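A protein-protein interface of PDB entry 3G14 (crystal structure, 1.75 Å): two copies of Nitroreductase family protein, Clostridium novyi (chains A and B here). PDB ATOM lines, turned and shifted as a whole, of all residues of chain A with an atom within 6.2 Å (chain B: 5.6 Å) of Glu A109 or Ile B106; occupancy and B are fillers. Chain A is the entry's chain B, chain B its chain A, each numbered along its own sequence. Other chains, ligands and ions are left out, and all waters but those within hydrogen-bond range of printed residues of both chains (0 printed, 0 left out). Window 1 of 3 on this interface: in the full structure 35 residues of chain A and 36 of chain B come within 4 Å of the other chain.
NE2 of His A110 is in hydrogen-bond range of OE2 of Glu B109 (2.6 Å). The side-chain carboxylate (OE2) of Glu A109 lies within hydrogen-bond range of a ring nitrogen (NE2) of His B110 (2.6 Å).
The side-chain carboxylate of Glu A109 lies within hydrogen-bond range of the indole nitrogen of Trp A124.
Among the printed residues, pairs that only touch across the chains: Arg A11 with Ala B37, Arg A11 with Pro B38, Ile A102 with Ala B105, Ala A105 with Ile B102, Ala A105 with Ala B105, Ile A106 with Glu B109, Glu A109 with Pro B38, Glu A109 with Ile B106, Leu A113 with His B110, Trp A124 with Pro B38, Trp A124 with Ile B102 and Trp A124 with Ile B106.
Of chain A, only Glu A109 (3.5 Å) and Trp A124 (3.4 Å) come within 4 Å of Ile B106. Of the printed residues of chain B, His A110 touches Glu B109 (2.6 Å). Of the printed residues of chain A, Pro B38 touches Arg A11 (3.6 Å), Glu A109 (3.2 Å) and Trp A124 (3.5 Å). Of the printed residues of chain B, Arg A11 touches Ala B37 (3.97 Å) and Pro B38 (3.6 Å). Of the printed residues of chain B, Ala A105 touches Ile B102 (3.4 Å) and Ala B105 (3.9 Å). Of the printed residues of chain A, Glu B109 touches Ile A106 (3.6 Å) and His A110 (2.6 Å). Val A112 touches none of the printed residues of chain B. Ser B39 touches none of the printed residues of chain A.
Of the 14 printed residues of chain B, 7 touch a printed residue of chain A. Hydrophobic or aromatic side chains of chain B within 4 Å of the printed part of chain A: Pro B38, Ile B102, Ala B105, Ile B106 and His B110. Of the 14 printed residues of chain A, 8 touch a printed residue of chain B. Printed residues of chain A that touch a printed residue of chain B: Arg A11, Ile A102, Ala A105, Ile A106, Glu A109, His A110, Leu A113 and Trp A124. Along chain A the printed residues that touch a printed residue of chain B span positions 11 to 124. Among the printed residues, no Asp or Glu carboxylate lies within 4 Å of a Lys or Arg side-chain nitrogen of the other chain.
Ile A102 touches Ala B105, and with the chains exchanged Ala A105 touches Ile B102. Ala B105 touches its own counterpart, Ala A105. Ile A106 touches Glu B109, and with the chains exchanged Glu A109 touches Ile B106. Glu A109 touches His B110, and with the chains exchanged His A110 touches Glu B109. 9 positions are printed for both chains. Of the 14 pairs that touch across the chains among the printed residues, 7 have their exchanged pair printed and touching as well.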
ATOM      1  N   ARG A  11     -23.012 -14.275  14.657  1.00  0.00           N
ATOM      2  CA  ARG A  11     -21.920 -15.107  15.127  1.00  0.00           C
ATOM      3  C   ARG A  11     -20.743 -15.039  14.168  1.00  0.00           C
ATOM      4  O   ARG A  11     -20.896 -15.279  12.989  1.00  0.00           O
ATOM      5  CB  ARG A  11     -22.339 -16.572  15.276  1.00  0.00           C
ATOM      6  CG  ARG A  11     -21.244 -17.442  15.900  1.00  0.00           C
ATOM      7  CD  ARG A  11     -21.183 -18.830  15.287  1.00  0.00           C
ATOM      8  NE  ARG A  11     -21.110 -18.825  13.838  1.00  0.00           N
ATOM      9  CZ  ARG A  11     -20.011 -18.599  13.114  1.00  0.00           C
ATOM     10  NH1 ARG A  11     -18.824 -18.316  13.684  1.00  0.00           N
ATOM     11  NH2 ARG A  11     -20.114 -18.645  11.793  1.00  0.00           N
ATOM     12  N   ILE A 102     -20.091 -35.983  18.166  1.00  0.00           N
ATOM     13  CA  ILE A 102     -21.332 -35.364  17.729  1.00  0.00           C
ATOM     14  C   ILE A 102     -21.988 -34.563  18.865  1.00  0.00           C
ATOM     15  O   ILE A 102     -22.316 -33.388  18.723  1.00  0.00           O
ATOM     16  CB  ILE A 102     -22.338 -36.422  17.210  1.00  0.00           C
ATOM     17  CG1 ILE A 102     -21.786 -37.071  15.923  1.00  0.00           C
ATOM     18  CG2 ILE A 102     -23.746 -35.757  17.039  1.00  0.00           C
ATOM     19  CD1 ILE A 102     -22.638 -38.222  15.315  1.00  0.00           C
ATOM     20  N   THR A 104     -20.871 -33.597  21.895  1.00  0.00           N
ATOM     21  CA  THR A 104     -20.093 -32.494  22.466  1.00  0.00           C
ATOM     22  C   THR A 104     -20.082 -31.314  21.475  1.00  0.00           C
ATOM     23  O   THR A 104     -20.161 -30.160  21.920  1.00  0.00           O
ATOM     24  CB  THR A 104     -18.651 -32.946  22.861  1.00  0.00           C
ATOM     25  OG1 THR A 104     -18.722 -34.113  23.681  1.00  0.00           O
ATOM     26  CG2 THR A 104     -17.880 -31.832  23.621  1.00  0.00           C
ATOM     27  N   ALA A 105     -20.005 -31.572  20.150  1.00  0.00           N
ATOM     28  CA  ALA A 105     -20.046 -30.468  19.144  1.00  0.00           C
ATOM     29  C   ALA A 105     -21.366 -29.673  19.229  1.00  0.00           C
ATOM     30  O   ALA A 105     -21.383 -28.409  19.186  1.00  0.00           O
ATOM     31  CB  ALA A 105     -19.827 -30.988  17.670  1.00  0.00           C
ATOM     32  N   ILE A 106     -22.450 -30.412  19.356  1.00  0.00           N
ATOM     33  CA  ILE A 106     -23.815 -29.844  19.489  1.00  0.00           C
ATOM     34  C   ILE A 106     -23.808 -28.889  20.662  1.00  0.00           C
ATOM     35  O   ILE A 106     -24.189 -27.720  20.544  1.00  0.00           O
ATOM     36  CB  ILE A 106     -24.907 -30.957  19.688  1.00  0.00           C
ATOM     37  CG1 ILE A 106     -25.091 -31.835  18.442  1.00  0.00           C
ATOM     38  CG2 ILE A 106     -26.300 -30.342  20.008  1.00  0.00           C
ATOM     39  CD1 ILE A 106     -26.012 -33.074  18.660  1.00  0.00           C
ATOM     40  N   ALA A 107     -23.361 -29.372  21.831  1.00  0.00           N
ATOM     41  CA  ALA A 107     -23.406 -28.570  23.064  1.00  0.00           C
ATOM     42  C   ALA A 107     -22.482 -27.365  22.998  1.00  0.00           C
ATOM     43  O   ALA A 107     -22.852 -26.258  23.431  1.00  0.00           O
ATOM     44  CB  ALA A 107     -23.091 -29.455  24.333  1.00  0.00           C
ATOM     45  N   MET A 108     -21.283 -27.564  22.459  1.00  0.00           N
ATOM     46  CA  MET A 108     -20.364 -26.454  22.255  1.00  0.00           C
ATOM     47  C   MET A 108     -20.930 -25.392  21.284  1.00  0.00           C
ATOM     48  O   MET A 108     -20.673 -24.205  21.471  1.00  0.00           O
ATOM     49  CB  MET A 108     -18.995 -26.970  21.755  1.00  0.00           C
ATOM     50  CG  MET A 108     -17.944 -25.896  21.715  1.00  0.00           C
ATOM     51  SD  MET A 108     -17.605 -24.983  23.481  1.00  0.00           S
ATOM     52  CE  MET A 108     -15.678 -25.514  23.416  1.00  0.00           C
ATOM     53  N   GLU A 109     -21.712 -25.780  20.274  1.00  0.00           N
ATOM     54  CA  GLU A 109     -22.320 -24.756  19.400  1.00  0.00           C
ATOM     55  C   GLU A 109     -23.416 -23.980  20.170  1.00  0.00           C
ATOM     56  O   GLU A 109     -23.668 -22.792  19.864  1.00  0.00           O
ATOM     57  CB  GLU A 109     -22.853 -25.356  18.091  1.00  0.00           C
ATOM     58  CG  GLU A 109     -23.340 -24.329  17.055  1.00  0.00           C
ATOM     59  CD  GLU A 109     -22.260 -23.361  16.579  1.00  0.00           C
ATOM     60  OE1 GLU A 109     -21.095 -23.486  17.074  1.00  0.00           O
ATOM     61  OE2 GLU A 109     -22.588 -22.487  15.740  1.00  0.00           O
ATOM     62  N   HIS A 110     -24.079 -24.624  21.142  1.00  0.00           N
ATOM     63  CA  HIS A 110     -24.995 -23.907  22.032  1.00  0.00           C
ATOM     64  C   HIS A 110     -24.224 -22.859  22.868  1.00  0.00           C
ATOM     65  O   HIS A 110     -24.711 -21.733  23.062  1.00  0.00           O
ATOM     66  CB  HIS A 110     -25.818 -24.879  22.933  1.00  0.00           C
ATOM     67  CG  HIS A 110     -26.950 -25.565  22.221  1.00  0.00           C
ATOM     68  ND1 HIS A 110     -28.173 -25.817  22.823  1.00  0.00           N
ATOM     69  CD2 HIS A 110     -27.020 -26.120  20.987  1.00  0.00           C
ATOM     70  CE1 HIS A 110     -28.961 -26.442  21.955  1.00  0.00           C
ATOM     71  NE2 HIS A 110     -28.283 -26.649  20.845  1.00  0.00           N
ATOM     72  N   ILE A 111     -23.021 -23.225  23.328  1.00  0.00           N
ATOM     73  CA  ILE A 111     -22.128 -22.272  24.065  1.00  0.00           C
ATOM     74  C   ILE A 111     -21.834 -21.077  23.173  1.00  0.00           C
ATOM     75  O   ILE A 111     -22.039 -19.907  23.559  1.00  0.00           O
ATOM     76  CB  ILE A 111     -20.768 -22.915  24.445  1.00  0.00           C
ATOM     77  CG1 ILE A 111     -20.950 -24.112  25.398  1.00  0.00           C
ATOM     78  CG2 ILE A 111     -19.813 -21.862  25.070  1.00  0.00           C
ATOM     79  CD1 ILE A 111     -21.370 -23.742  26.784  1.00  0.00           C
ATOM     80  N   VAL A 112     -21.350 -21.392  21.974  1.00  0.00           N
ATOM     81  CA  VAL A 112     -20.941 -20.381  20.989  1.00  0.00           C
ATOM     82  C   VAL A 112     -22.105 -19.466  20.597  1.00  0.00           C
ATOM     83  O   VAL A 112     -21.996 -18.230  20.647  1.00  0.00           O
ATOM     84  CB  VAL A 112     -20.249 -21.065  19.761  1.00  0.00           C
ATOM     85  CG1 VAL A 112     -20.220 -20.139  18.520  1.00  0.00           C
ATOM     86  CG2 VAL A 112     -18.860 -21.582  20.153  1.00  0.00           C
ATOM     87  N   LEU A 113     -23.236 -20.057  20.219  1.00  0.00           N
ATOM     88  CA  LEU A 113     -24.379 -19.226  19.873  1.00  0.00           C
ATOM     89  C   LEU A 113     -24.942 -18.454  21.072  1.00  0.00           C
ATOM     90  O   LEU A 113     -25.364 -17.283  20.961  1.00  0.00           O
ATOM     91  CB  LEU A 113     -25.450 -20.073  19.215  1.00  0.00           C
ATOM     92  CG  LEU A 113     -25.097 -20.676  17.877  1.00  0.00           C
ATOM     93  CD1 LEU A 113     -26.182 -21.672  17.520  1.00  0.00           C
ATOM     94  CD2 LEU A 113     -24.907 -19.559  16.768  1.00  0.00           C
ATOM     95  N   GLY A 114     -24.965 -19.091  22.232  1.00  0.00           N
ATOM     96  CA  GLY A 114     -25.404 -18.409  23.433  1.00  0.00           C
ATOM     97  C   GLY A 114     -24.515 -17.229  23.816  1.00  0.00           C
ATOM     98  O   GLY A 114     -25.019 -16.168  24.203  1.00  0.00           O
ATOM     99  N   TRP A 124     -14.015 -21.017  17.723  1.00  0.00           N
ATOM    100  CA  TRP A 124     -13.758 -22.477  17.814  1.00  0.00           C
ATOM    101  C   TRP A 124     -12.295 -22.802  17.669  1.00  0.00           C
ATOM    102  O   TRP A 124     -11.659 -22.433  16.692  1.00  0.00           O
ATOM    103  CB  TRP A 124     -14.527 -23.222  16.742  1.00  0.00           C
ATOM    104  CG  TRP A 124     -15.927 -23.572  17.064  1.00  0.00           C
ATOM    105  CD1 TRP A 124     -17.044 -22.809  16.839  1.00  0.00           C
ATOM    106  CD2 TRP A 124     -16.397 -24.843  17.528  1.00  0.00           C
ATOM    107  NE1 TRP A 124     -18.179 -23.498  17.207  1.00  0.00           N
ATOM    108  CE2 TRP A 124     -17.813 -24.743  17.656  1.00  0.00           C
ATOM    109  CE3 TRP A 124     -15.766 -26.019  17.914  1.00  0.00           C
ATOM    110  CZ2 TRP A 124     -18.603 -25.803  18.116  1.00  0.00           C
ATOM    111  CZ3 TRP A 124     -16.562 -27.097  18.351  1.00  0.00           C
ATOM    112  CH2 TRP A 124     -17.963 -26.969  18.446  1.00  0.00           C
ATOM    113  N   ALA B  37     -23.048 -21.779   9.663  1.00  0.00           N
ATOM    114  CA  ALA B  37     -22.390 -22.511  10.766  1.00  0.00           C
ATOM    115  C   ALA B  37     -20.864 -22.375  10.663  1.00  0.00           C
ATOM    116  O   ALA B  37     -20.313 -22.322   9.550  1.00  0.00           O
ATOM    117  CB  ALA B  37     -22.785 -23.953  10.733  1.00  0.00           C
ATOM    118  N   PRO B  38     -20.156 -22.343  11.815  1.00  0.00           N
ATOM    119  CA  PRO B  38     -18.700 -22.347  11.746  1.00  0.00           C
ATOM    120  C   PRO B  38     -18.199 -23.729  11.382  1.00  0.00           C
ATOM    121  O   PRO B  38     -18.870 -24.719  11.643  1.00  0.00           O
ATOM    122  CB  PRO B  38     -18.289 -21.999  13.182  1.00  0.00           C
ATOM    123  CG  PRO B  38     -19.386 -22.641  14.016  1.00  0.00           C
ATOM    124  CD  PRO B  38     -20.626 -22.354  13.214  1.00  0.00           C
ATOM    125  N   SER B  39     -17.043 -23.801  10.751  1.00  0.00           N
ATOM    126  CA  SER B  39     -16.415 -25.101  10.488  1.00  0.00           C
ATOM    127  C   SER B  39     -14.910 -24.939  10.497  1.00  0.00           C
ATOM    128  O   SER B  39     -14.387 -23.841  10.357  1.00  0.00           O
ATOM    129  CB  SER B  39     -16.851 -25.658   9.121  1.00  0.00           C
ATOM    130  OG  SER B  39     -16.468 -24.759   8.077  1.00  0.00           O
ATOM    131  N   LEU B 101     -17.242 -35.131  11.829  1.00  0.00           N
ATOM    132  CA  LEU B 101     -18.308 -35.357  12.806  1.00  0.00           C
ATOM    133  C   LEU B 101     -18.627 -34.076  13.583  1.00  0.00           C
ATOM    134  O   LEU B 101     -19.794 -33.722  13.717  1.00  0.00           O
ATOM    135  CB  LEU B 101     -17.983 -36.505  13.774  1.00  0.00           C
ATOM    136  CG  LEU B 101     -18.041 -37.898  13.133  1.00  0.00           C
ATOM    137  CD1 LEU B 101     -17.422 -38.934  14.070  1.00  0.00           C
ATOM    138  CD2 LEU B 101     -19.480 -38.268  12.709  1.00  0.00           C
ATOM    139  N   ILE B 102     -17.589 -33.366  14.023  1.00  0.00           N
ATOM    140  CA  ILE B 102     -17.773 -32.127  14.738  1.00  0.00           C
ATOM    141  C   ILE B 102     -18.517 -31.123  13.872  1.00  0.00           C
ATOM    142  O   ILE B 102     -19.573 -30.583  14.280  1.00  0.00           O
ATOM    143  CB  ILE B 102     -16.413 -31.553  15.220  1.00  0.00           C
ATOM    144  CG1 ILE B 102     -15.809 -32.479  16.314  1.00  0.00           C
ATOM    145  CG2 ILE B 102     -16.613 -30.064  15.716  1.00  0.00           C
ATOM    146  CD1 ILE B 102     -14.291 -32.261  16.568  1.00  0.00           C
ATOM    147  N   ASP B 103     -17.990 -30.909  12.659  1.00  0.00           N
ATOM    148  CA  ASP B 103     -18.508 -29.872  11.736  1.00  0.00           C
ATOM    149  C   ASP B 103     -19.914 -30.169  11.236  1.00  0.00           C
ATOM    150  O   ASP B 103     -20.774 -29.270  11.242  1.00  0.00           O
ATOM    151  CB  ASP B 103     -17.504 -29.598  10.614  1.00  0.00           C
ATOM    152  CG  ASP B 103     -16.305 -28.774  11.148  1.00  0.00           C
ATOM    153  OD1 ASP B 103     -16.341 -28.435  12.333  1.00  0.00           O
ATOM    154  OD2 ASP B 103     -15.373 -28.498  10.468  1.00  0.00           O
ATOM    155  N   THR B 104     -20.163 -31.424  10.891  1.00  0.00           N
ATOM    156  CA  THR B 104     -21.494 -31.818  10.432  1.00  0.00           C
ATOM    157  C   THR B 104     -22.527 -31.676  11.582  1.00  0.00           C
ATOM    158  O   THR B 104     -23.654 -31.190  11.374  1.00  0.00           O
ATOM    159  CB  THR B 104     -21.493 -33.215   9.797  1.00  0.00           C
ATOM    160  OG1 THR B 104     -20.513 -33.258   8.749  1.00  0.00           O
ATOM    161  CG2 THR B 104     -22.882 -33.557   9.160  1.00  0.00           C
ATOM    162  N   ALA B 105     -22.132 -32.055  12.795  1.00  0.00           N
ATOM    163  CA  ALA B 105     -23.020 -31.949  13.969  1.00  0.00           C
ATOM    164  C   ALA B 105     -23.419 -30.493  14.274  1.00  0.00           C
ATOM    165  O   ALA B 105     -24.596 -30.198  14.572  1.00  0.00           O
ATOM    166  CB  ALA B 105     -22.360 -32.597  15.254  1.00  0.00           C
ATOM    167  N   ILE B 106     -22.431 -29.609  14.214  1.00  0.00           N
ATOM    168  CA  ILE B 106     -22.637 -28.138  14.339  1.00  0.00           C
ATOM    169  C   ILE B 106     -23.707 -27.684  13.357  1.00  0.00           C
ATOM    170  O   ILE B 106     -24.735 -27.118  13.762  1.00  0.00           O
ATOM    171  CB  ILE B 106     -21.318 -27.350  14.134  1.00  0.00           C
ATOM    172  CG1 ILE B 106     -20.300 -27.609  15.237  1.00  0.00           C
ATOM    173  CG2 ILE B 106     -21.570 -25.812  14.151  1.00  0.00           C
ATOM    174  CD1 ILE B 106     -18.913 -26.971  14.902  1.00  0.00           C
ATOM    175  N   ALA B 107     -23.534 -28.002  12.068  1.00  0.00           N
ATOM    176  CA  ALA B 107     -24.465 -27.531  11.053  1.00  0.00           C
ATOM    177  C   ALA B 107     -25.848 -28.188  11.220  1.00  0.00           C
ATOM    178  O   ALA B 107     -26.863 -27.509  11.098  1.00  0.00           O
ATOM    179  CB  ALA B 107     -23.923 -27.774   9.628  1.00  0.00           C
ATOM    180  N   MET B 108     -25.886 -29.488  11.513  1.00  0.00           N
ATOM    181  CA  MET B 108     -27.181 -30.153  11.783  1.00  0.00           C
ATOM    182  C   MET B 108     -27.942 -29.494  12.971  1.00  0.00           C
ATOM    183  O   MET B 108     -29.163 -29.372  12.943  1.00  0.00           O
ATOM    184  CB  MET B 108     -26.992 -31.666  12.014  1.00  0.00           C
ATOM    185  CG  MET B 108     -28.299 -32.435  12.138  1.00  0.00           C
ATOM    186  SD  MET B 108     -29.478 -32.217  10.550  1.00  0.00           S
ATOM    187  CE  MET B 108     -29.667 -34.140  10.116  1.00  0.00           C
ATOM    188  N   GLU B 109     -27.232 -29.043  13.998  1.00  0.00           N
ATOM    189  CA  GLU B 109     -27.882 -28.374  15.100  1.00  0.00           C
ATOM    190  C   GLU B 109     -28.440 -26.995  14.695  1.00  0.00           C
ATOM    191  O   GLU B 109     -29.469 -26.545  15.247  1.00  0.00           O
ATOM    192  CB  GLU B 109     -26.955 -28.285  16.317  1.00  0.00           C
ATOM    193  CG  GLU B 109     -27.638 -27.803  17.625  1.00  0.00           C
ATOM    194  CD  GLU B 109     -28.806 -28.637  18.125  1.00  0.00           C
ATOM    195  OE1 GLU B 109     -29.132 -29.646  17.456  1.00  0.00           O
ATOM    196  OE2 GLU B 109     -29.408 -28.253  19.198  1.00  0.00           O
ATOM    197  N   HIS B 110     -27.775 -26.315  13.763  1.00  0.00           N
ATOM    198  CA  HIS B 110     -28.330 -25.093  13.159  1.00  0.00           C
ATOM    199  C   HIS B 110     -29.679 -25.410  12.416  1.00  0.00           C
ATOM    200  O   HIS B 110     -30.630 -24.630  12.514  1.00  0.00           O
ATOM    201  CB  HIS B 110     -27.312 -24.422  12.243  1.00  0.00           C
ATOM    202  CG  HIS B 110     -26.253 -23.640  12.953  1.00  0.00           C
ATOM    203  ND1 HIS B 110     -25.810 -22.427  12.489  1.00  0.00           N
ATOM    204  CD2 HIS B 110     -25.555 -23.880  14.093  1.00  0.00           C
ATOM    205  CE1 HIS B 110     -24.885 -21.949  13.307  1.00  0.00           C
ATOM    206  NE2 HIS B 110     -24.703 -22.814  14.283  1.00  0.00           N
ATOM    207  N   ILE B 111     -29.776 -26.540  11.723  1.00  0.00           N
ATOM    208  CA  ILE B 111     -31.050 -26.917  11.064  1.00  0.00           C
ATOM    209  C   ILE B 111     -32.091 -27.288  12.131  1.00  0.00           C
ATOM    210  O   ILE B 111     -33.251 -26.882  12.032  1.00  0.00           O
ATOM    211  CB  ILE B 111     -30.866 -28.041  10.029  1.00  0.00           C
ATOM    212  CG1 ILE B 111     -30.238 -27.467   8.743  1.00  0.00           C
ATOM    213  CG2 ILE B 111     -32.220 -28.700   9.695  1.00  0.00           C
ATOM    214  CD1 ILE B 111     -29.484 -28.494   7.901  1.00  0.00           C
